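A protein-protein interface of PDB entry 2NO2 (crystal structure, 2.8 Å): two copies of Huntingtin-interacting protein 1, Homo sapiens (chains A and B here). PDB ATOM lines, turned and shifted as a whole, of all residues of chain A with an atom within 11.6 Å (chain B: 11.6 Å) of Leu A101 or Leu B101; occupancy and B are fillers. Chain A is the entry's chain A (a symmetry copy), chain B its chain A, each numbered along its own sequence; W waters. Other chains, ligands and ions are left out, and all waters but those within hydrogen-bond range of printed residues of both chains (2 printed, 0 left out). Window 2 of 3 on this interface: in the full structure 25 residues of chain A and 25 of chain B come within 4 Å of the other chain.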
ATOM      1  N   ALA A  92     -15.345 -11.101  15.728  1.00  0.00           N
ATOM      2  CA  ALA A  92     -16.267 -11.711  16.665  1.00  0.00           C
ATOM      3  C   ALA A  92     -15.528 -12.322  17.841  1.00  0.00           C
ATOM      4  O   ALA A  92     -15.895 -12.076  18.983  1.00  0.00           O
ATOM      5  CB  ALA A  92     -17.102 -12.763  15.963  1.00  0.00           C
ATOM      6  N   GLU A  93     -14.481 -13.101  17.563  1.00  0.00           N
ATOM      7  CA  GLU A  93     -13.710 -13.752  18.613  1.00  0.00           C
ATOM      8  C   GLU A  93     -13.103 -12.761  19.593  1.00  0.00           C
ATOM      9  O   GLU A  93     -13.159 -12.968  20.823  1.00  0.00           O
ATOM     10  CB  GLU A  93     -12.611 -14.623  18.009  1.00  0.00           C
ATOM     11  CG  GLU A  93     -13.039 -16.056  17.856  1.00  0.00           C
ATOM     12  CD  GLU A  93     -13.717 -16.566  19.109  1.00  0.00           C
ATOM     13  OE1 GLU A  93     -13.064 -16.606  20.180  1.00  0.00           O
ATOM     14  OE2 GLU A  93     -14.912 -16.912  19.024  1.00  0.00           O
ATOM     15  N   LEU A  94     -12.525 -11.683  19.050  1.00  0.00           N
ATOM     16  CA  LEU A  94     -11.900 -10.658  19.886  1.00  0.00           C
ATOM     17  C   LEU A  94     -12.981 -10.056  20.772  1.00  0.00           C
ATOM     18  O   LEU A  94     -12.778  -9.870  21.976  1.00  0.00           O
ATOM     19  CB  LEU A  94     -11.266  -9.571  19.013  1.00  0.00           C
ATOM     20  CG  LEU A  94      -9.816  -9.191  19.314  1.00  0.00           C
ATOM     21  CD1 LEU A  94      -9.714  -8.674  20.715  1.00  0.00           C
ATOM     22  CD2 LEU A  94      -8.910 -10.399  19.154  1.00  0.00           C
ATOM     23  N   GLU A  95     -14.142  -9.770  20.175  1.00  0.00           N
ATOM     24  CA  GLU A  95     -15.253  -9.192  20.920  1.00  0.00           C
ATOM     25  C   GLU A  95     -15.634 -10.095  22.082  1.00  0.00           C
ATOM     26  O   GLU A  95     -15.738  -9.625  23.212  1.00  0.00           O
ATOM     27  CB  GLU A  95     -16.458  -8.968  20.008  1.00  0.00           C
ATOM     28  CG  GLU A  95     -17.701  -8.471  20.738  1.00  0.00           C
ATOM     29  CD  GLU A  95     -18.797  -8.047  19.780  1.00  0.00           C
ATOM     30  OE1 GLU A  95     -18.819  -8.555  18.637  1.00  0.00           O
ATOM     31  OE2 GLU A  95     -19.643  -7.216  20.170  1.00  0.00           O
ATOM     32  N   LYS A  96     -15.828 -11.386  21.808  1.00  0.00           N
ATOM     33  CA  LYS A  96     -16.171 -12.357  22.840  1.00  0.00           C
ATOM     34  C   LYS A  96     -15.165 -12.258  23.996  1.00  0.00           C
ATOM     35  O   LYS A  96     -15.560 -12.201  25.151  1.00  0.00           O
ATOM     36  CB  LYS A  96     -16.154 -13.765  22.255  1.00  0.00           C
ATOM     37  CG  LYS A  96     -16.548 -14.849  23.227  1.00  0.00           C
ATOM     38  CD  LYS A  96     -16.274 -16.206  22.615  1.00  0.00           C
ATOM     39  CE  LYS A  96     -16.714 -17.342  23.521  1.00  0.00           C
ATOM     40  NZ  LYS A  96     -16.254 -18.674  23.010  1.00  0.00           N
ATOM     41  N   GLU A  97     -13.868 -12.231  23.685  1.00  0.00           N
ATOM     42  CA  GLU A  97     -12.833 -12.107  24.719  1.00  0.00           C
ATOM     43  C   GLU A  97     -12.956 -10.789  25.487  1.00  0.00           C
ATOM     44  O   GLU A  97     -12.977 -10.792  26.722  1.00  0.00           O
ATOM     45  CB  GLU A  97     -11.436 -12.174  24.099  1.00  0.00           C
ATOM     46  CG  GLU A  97     -11.009 -13.548  23.631  1.00  0.00           C
ATOM     47  CD  GLU A  97      -9.667 -13.524  22.942  1.00  0.00           C
ATOM     48  OE1 GLU A  97      -8.746 -12.873  23.473  1.00  0.00           O
ATOM     49  OE2 GLU A  97      -9.533 -14.158  21.875  1.00  0.00           O
ATOM     50  N   ARG A  98     -13.015  -9.674  24.751  1.00  0.00           N
ATOM     51  CA  ARG A  98     -13.142  -8.341  25.339  1.00  0.00           C
ATOM     52  C   ARG A  98     -14.329  -8.308  26.307  1.00  0.00           C
ATOM     53  O   ARG A  98     -14.230  -7.761  27.407  1.00  0.00           O
ATOM     54  CB  ARG A  98     -13.341  -7.302  24.231  1.00  0.00           C
ATOM     55  CG  ARG A  98     -13.221  -5.842  24.673  1.00  0.00           C
ATOM     56  CD  ARG A  98     -14.455  -5.334  25.407  1.00  0.00           C
ATOM     57  NE  ARG A  98     -15.666  -5.348  24.579  1.00  0.00           N
ATOM     58  CZ  ARG A  98     -15.914  -4.521  23.561  1.00  0.00           C
ATOM     59  NH1 ARG A  98     -15.035  -3.587  23.219  1.00  0.00           N
ATOM     60  NH2 ARG A  98     -17.050  -4.625  22.881  1.00  0.00           N
ATOM     61  N   ASP A  99     -15.454  -8.896  25.902  1.00  0.00           N
ATOM     62  CA  ASP A  99     -16.634  -8.926  26.759  1.00  0.00           C
ATOM     63  C   ASP A  99     -16.376  -9.743  28.006  1.00  0.00           C
ATOM     64  O   ASP A  99     -16.852  -9.384  29.076  1.00  0.00           O
ATOM     65  CB  ASP A  99     -17.834  -9.501  26.019  1.00  0.00           C
ATOM     66  CG  ASP A  99     -18.258  -8.647  24.844  1.00  0.00           C
ATOM     67  OD1 ASP A  99     -18.020  -7.417  24.884  1.00  0.00           O
ATOM     68  OD2 ASP A  99     -18.842  -9.201  23.885  1.00  0.00           O
ATOM     69  N   SER A 100     -15.632 -10.844  27.867  1.00  0.00           N
ATOM     70  CA  SER A 100     -15.280 -11.710  28.999  1.00  0.00           C
ATOM     71  C   SER A 100     -14.463 -10.959  30.032  1.00  0.00           C
ATOM     72  O   SER A 100     -14.673 -11.117  31.226  1.00  0.00           O
ATOM     73  CB  SER A 100     -14.455 -12.898  28.537  1.00  0.00           C
ATOM     74  OG  SER A 100     -15.232 -13.718  27.704  1.00  0.00           O
ATOM     75  N   LEU A 101     -13.518 -10.154  29.568  1.00  0.00           N
ATOM     76  CA  LEU A 101     -12.686  -9.392  30.475  1.00  0.00           C
ATOM     77  C   LEU A 101     -13.411  -8.210  31.126  1.00  0.00           C
ATOM     78  O   LEU A 101     -13.061  -7.802  32.235  1.00  0.00           O
ATOM     79  CB  LEU A 101     -11.429  -8.898  29.752  1.00  0.00           C
ATOM     80  CG  LEU A 101     -10.307  -9.890  29.430  1.00  0.00           C
ATOM     81  CD1 LEU A 101     -10.017 -10.745  30.643  1.00  0.00           C
ATOM     82  CD2 LEU A 101     -10.703 -10.761  28.271  1.00  0.00           C
ATOM     83  N   VAL A 102     -14.412  -7.647  30.463  1.00  0.00           N
ATOM     84  CA  VAL A 102     -15.115  -6.512  31.057  1.00  0.00           C
ATOM     85  C   VAL A 102     -16.398  -6.976  31.752  1.00  0.00           C
ATOM     86  O   VAL A 102     -16.689  -8.196  31.726  1.00  0.00           O
ATOM     87  CB  VAL A 102     -15.444  -5.422  29.991  1.00  0.00           C
ATOM     88  CG1 VAL A 102     -16.061  -4.216  30.645  1.00  0.00           C
ATOM     89  CG2 VAL A 102     -14.178  -4.986  29.284  1.00  0.00           C
ATOM     90  N   ALA B  92      -8.232  -3.410  15.060  1.00  0.00           N
ATOM     91  CA  ALA B  92      -7.119  -2.832  15.786  1.00  0.00           C
ATOM     92  C   ALA B  92      -7.570  -2.270  17.121  1.00  0.00           C
ATOM     93  O   ALA B  92      -6.954  -2.557  18.140  1.00  0.00           O
ATOM     94  CB  ALA B  92      -6.460  -1.750  14.954  1.00  0.00           C
ATOM     95  N   GLU B  93      -8.649  -1.485  17.117  1.00  0.00           N
ATOM     96  CA  GLU B  93      -9.159  -0.878  18.339  1.00  0.00           C
ATOM     97  C   GLU B  93      -9.534  -1.908  19.392  1.00  0.00           C
ATOM     98  O   GLU B  93      -9.199  -1.748  20.585  1.00  0.00           O
ATOM     99  CB  GLU B  93     -10.363   0.011  18.033  1.00  0.00           C
ATOM    100  CG  GLU B  93      -9.975   1.450  17.841  1.00  0.00           C
ATOM    101  CD  GLU B  93      -9.029   1.916  18.927  1.00  0.00           C
ATOM    102  OE1 GLU B  93      -9.421   1.912  20.118  1.00  0.00           O
ATOM    103  OE2 GLU B  93      -7.882   2.270  18.586  1.00  0.00           O
ATOM    104  N   LEU B  94     -10.224  -2.967  18.954  1.00  0.00           N
ATOM    105  CA  LEU B  94     -10.648  -4.025  19.870  1.00  0.00           C
ATOM    106  C   LEU B  94      -9.396  -4.656  20.465  1.00  0.00           C
ATOM    107  O   LEU B  94      -9.323  -4.889  21.675  1.00  0.00           O
ATOM    108  CB  LEU B  94     -11.468  -5.082  19.123  1.00  0.00           C
ATOM    109  CG  LEU B  94     -12.814  -5.479  19.730  1.00  0.00           C
ATOM    110  CD1 LEU B  94     -12.598  -6.049  21.097  1.00  0.00           C
ATOM    111  CD2 LEU B  94     -13.727  -4.270  19.825  1.00  0.00           C
ATOM    112  N   GLU B  95      -8.402  -4.914  19.610  1.00  0.00           N
ATOM    113  CA  GLU B  95      -7.154  -5.515  20.061  1.00  0.00           C
ATOM    114  C   GLU B  95      -6.516  -4.656  21.140  1.00  0.00           C
ATOM    115  O   GLU B  95      -6.160  -5.168  22.199  1.00  0.00           O
ATOM    116  CB  GLU B  95      -6.188  -5.699  18.892  1.00  0.00           C
ATOM    117  CG  GLU B  95      -4.814  -6.218  19.302  1.00  0.00           C
ATOM    118  CD  GLU B  95      -3.965  -6.600  18.106  1.00  0.00           C
ATOM    119  OE1 GLU B  95      -4.201  -6.050  17.008  1.00  0.00           O
ATOM    120  OE2 GLU B  95      -3.057  -7.443  18.262  1.00  0.00           O
ATOM    121  N   LYS B  96      -6.383  -3.354  20.878  1.00  0.00           N
ATOM    122  CA  LYS B  96      -5.811  -2.422  21.842  1.00  0.00           C
ATOM    123  C   LYS B  96      -6.529  -2.569  23.191  1.00  0.00           C
ATOM    124  O   LYS B  96      -5.883  -2.668  24.224  1.00  0.00           O
ATOM    125  CB  LYS B  96      -5.955  -0.992  21.331  1.00  0.00           C
ATOM    126  CG  LYS B  96      -5.345   0.056  22.228  1.00  0.00           C
ATOM    127  CD  LYS B  96      -5.745   1.434  21.746  1.00  0.00           C
ATOM    128  CE  LYS B  96      -5.107   2.536  22.572  1.00  0.00           C
ATOM    129  NZ  LYS B  96      -5.665   3.885  22.229  1.00  0.00           N
ATOM    130  N   GLU B  97      -7.863  -2.589  23.182  1.00  0.00           N
ATOM    131  CA  GLU B  97      -8.638  -2.757  24.417  1.00  0.00           C
ATOM    132  C   GLU B  97      -8.350  -4.103  25.087  1.00  0.00           C
ATOM    133  O   GLU B  97      -8.050  -4.146  26.284  1.00  0.00           O
ATOM    134  CB  GLU B  97     -10.139  -2.673  24.133  1.00  0.00           C
ATOM    135  CG  GLU B  97     -10.655  -1.284  23.827  1.00  0.00           C
ATOM    136  CD  GLU B  97     -12.118  -1.288  23.459  1.00  0.00           C
ATOM    137  OE1 GLU B  97     -12.897  -1.962  24.159  1.00  0.00           O
ATOM    138  OE2 GLU B  97     -12.487  -0.614  22.475  1.00  0.00           O
ATOM    139  N   ARG B  98      -8.464  -5.189  24.315  1.00  0.00           N
ATOM    140  CA  ARG B  98      -8.213  -6.543  24.808  1.00  0.00           C
ATOM    141  C   ARG B  98      -6.838  -6.607  25.480  1.00  0.00           C
ATOM    142  O   ARG B  98      -6.687  -7.197  26.552  1.00  0.00           O
ATOM    143  CB  ARG B  98      -8.274  -7.538  23.645  1.00  0.00           C
ATOM    144  CG  ARG B  98      -8.298  -9.014  24.046  1.00  0.00           C
ATOM    145  CD  ARG B  98      -6.931  -9.544  24.462  1.00  0.00           C
ATOM    146  NE  ARG B  98      -5.940  -9.494  23.383  1.00  0.00           N
ATOM    147  CZ  ARG B  98      -5.932 -10.281  22.305  1.00  0.00           C
ATOM    148  NH1 ARG B  98      -6.870 -11.205  22.135  1.00  0.00           N
ATOM    149  NH2 ARG B  98      -4.979 -10.146  21.390  1.00  0.00           N
ATOM    150  N   ASP B  99      -5.831  -6.000  24.853  1.00  0.00           N
ATOM    151  CA  ASP B  99      -4.488  -5.997  25.421  1.00  0.00           C
ATOM    152  C   ASP B  99      -4.453  -5.229  26.724  1.00  0.00           C
ATOM    153  O   ASP B  99      -3.749  -5.626  27.645  1.00  0.00           O
ATOM    154  CB  ASP B  99      -3.484  -5.389  24.452  1.00  0.00           C
ATOM    155  CG  ASP B  99      -3.341  -6.196  23.179  1.00  0.00           C
ATOM    156  OD1 ASP B  99      -3.569  -7.427  23.225  1.00  0.00           O
ATOM    157  OD2 ASP B  99      -2.987  -5.603  22.134  1.00  0.00           O
ATOM    158  N   SER B 100      -5.204  -4.127  26.800  1.00  0.00           N
ATOM    159  CA  SER B 100      -5.287  -3.306  28.014  1.00  0.00           C
ATOM    160  C   SER B 100      -5.852  -4.099  29.176  1.00  0.00           C
ATOM    161  O   SER B 100      -5.376  -3.986  30.296  1.00  0.00           O
ATOM    162  CB  SER B 100      -6.190  -2.105  27.796  1.00  0.00           C
ATOM    163  OG  SER B 100      -5.618  -1.251  26.841  1.00  0.00           O
ATOM    164  N   LEU B 101      -6.882  -4.891  28.907  1.00  0.00           N
ATOM    165  CA  LEU B 101      -7.489  -5.690  29.949  1.00  0.00           C
ATOM    166  C   LEU B 101      -6.641  -6.893  30.375  1.00  0.00           C
ATOM    167  O   LEU B 101      -6.733  -7.344  31.517  1.00  0.00           O
ATOM    168  CB  LEU B 101      -8.880  -6.161  29.512  1.00  0.00           C
ATOM    169  CG  LEU B 101     -10.041  -5.163  29.490  1.00  0.00           C
ATOM    170  CD1 LEU B 101     -10.045  -4.356  30.770  1.00  0.00           C
ATOM    171  CD2 LEU B 101      -9.914  -4.247  28.305  1.00  0.00           C
ATOM    172  N   VAL B 102      -5.819  -7.426  29.481  1.00  0.00           N
ATOM    173  CA  VAL B 102      -5.005  -8.579  29.857  1.00  0.00           C
ATOM    174  C   VAL B 102      -3.595  -8.137  30.260  1.00  0.00           C
ATOM    175  O   VAL B 102      -3.312  -6.915  30.216  1.00  0.00           O
ATOM    176  CB  VAL B 102      -4.931  -9.627  28.703  1.00  0.00           C
ATOM    177  CG1 VAL B 102      -4.186 -10.853  29.154  1.00  0.00           C
ATOM    178  CG2 VAL B 102      -6.325 -10.041  28.285  1.00  0.00           C
HETATM  179  O   HOH W   1      -6.698 -14.301  21.135  1.00  0.00           O
HETATM  180  O   HOH W   2     -15.416  -0.455  22.403  1.00  0.00           O
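OE1 of Glu B97 lies within salt-bridge range of NH1 of Arg A98 (2.8 Å).
OE1 of Glu A97 lies within salt-bridge range of NH1 of Arg B98.
NE of Arg B98 is in salt-bridge range of OD1 of Asp B99.
The guanidinium group (NE) of Arg A98 lies within salt-bridge range of the side-chain carboxylate (OD1) of Asp A99 (3.1 Å).
CD1 of Leu A94 touches CD1 of Leu B94 (3.9 Å).
Arg B98 touches Leu A94 (CB to CD1, 3.5 Å).
Arg A98 touches Leu B94 (CB to CD1, 3.5 Å).
Leu B101 touches Leu A101 (CB to CB, 3.7 Å).
Of chain B, only Leu B101 comes within 4 Å of Leu A101.
Of chain A, only Leu A101 comes within 4 Å of Leu B101.
Glu A97 touches just one residue of chain B: Arg B98 (2.8 Å).
No residue of chain B comes within 4 Å of Ser A100.
No residue of chain B comes within 4 Å of Val A102.
Of the printed residues of chain A, Glu B97 touches Arg A98 (2.8 Å).
Val B102 touches none of the printed residues of chain A.
Of the printed residues of chain B, Leu A94 touches Leu B94 (3.9 Å) and Arg B98 (3.5 Å).
Of the printed residues of chain B, Arg A98 touches Leu B94 (3.5 Å) and Glu B97 (2.8 Å).
Printed residues of chain A within 4 Å of Arg B98: Leu A94 (3.5 Å) and Glu A97 (2.8 Å).
The nearest residue of chain B that does not touch Leu A101 is Val B102 (4.1 Å).
The nearest residue of chain A that does not touch Leu B101 is Val A102 (4.1 Å).
Of the 11 printed residues of chain B, 4 touch a printed residue of chain A.
Printed residues of chain B that touch a printed residue of chain A: Leu B94, Glu B97, Arg B98 and Leu B101.
Hydrophobic or aromatic side chains of chain B within 4 Å of the printed part of chain A: Leu B94 and Leu B101.
Printed residues of chain A that touch a printed residue of chain B: Leu A94, Glu A97, Arg A98 and Leu A101.
Hydrophobic or aromatic side chains of chain A within 4 Å of the printed part of chain B: Leu A94 and Leu A101.
Among the printed residues, 6 pairs touch across the chains.
Among the printed residues, Asp or Glu carboxylates within 4 Å of a Lys or Arg side-chain nitrogen of the other chain: Glu A97 with Arg B98 and Arg A98 with Glu B97.
Leu B94 touches its own counterpart, Leu A94.
Leu A94 touches Arg B98, and with the chains exchanged Arg A98 touches Leu B94.
Glu A97 touches Arg B98, and with the chains exchanged Arg A98 touches Glu B97.
Leu B101 touches its own counterpart, Leu A101.
Of the 6 pairs that touch across the chains among the printed residues, 6 have their exchanged pair printed and touching as well.
Water W2 bridges OE2 of Glu B97 (2.9 Å) and NH1 of Arg A98 (3.3 Å).
Water W1 bridges the side-chain carboxylate of Glu A97 (2.9 Å) and the guanidinium group of Arg B98 (3.3 Å).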
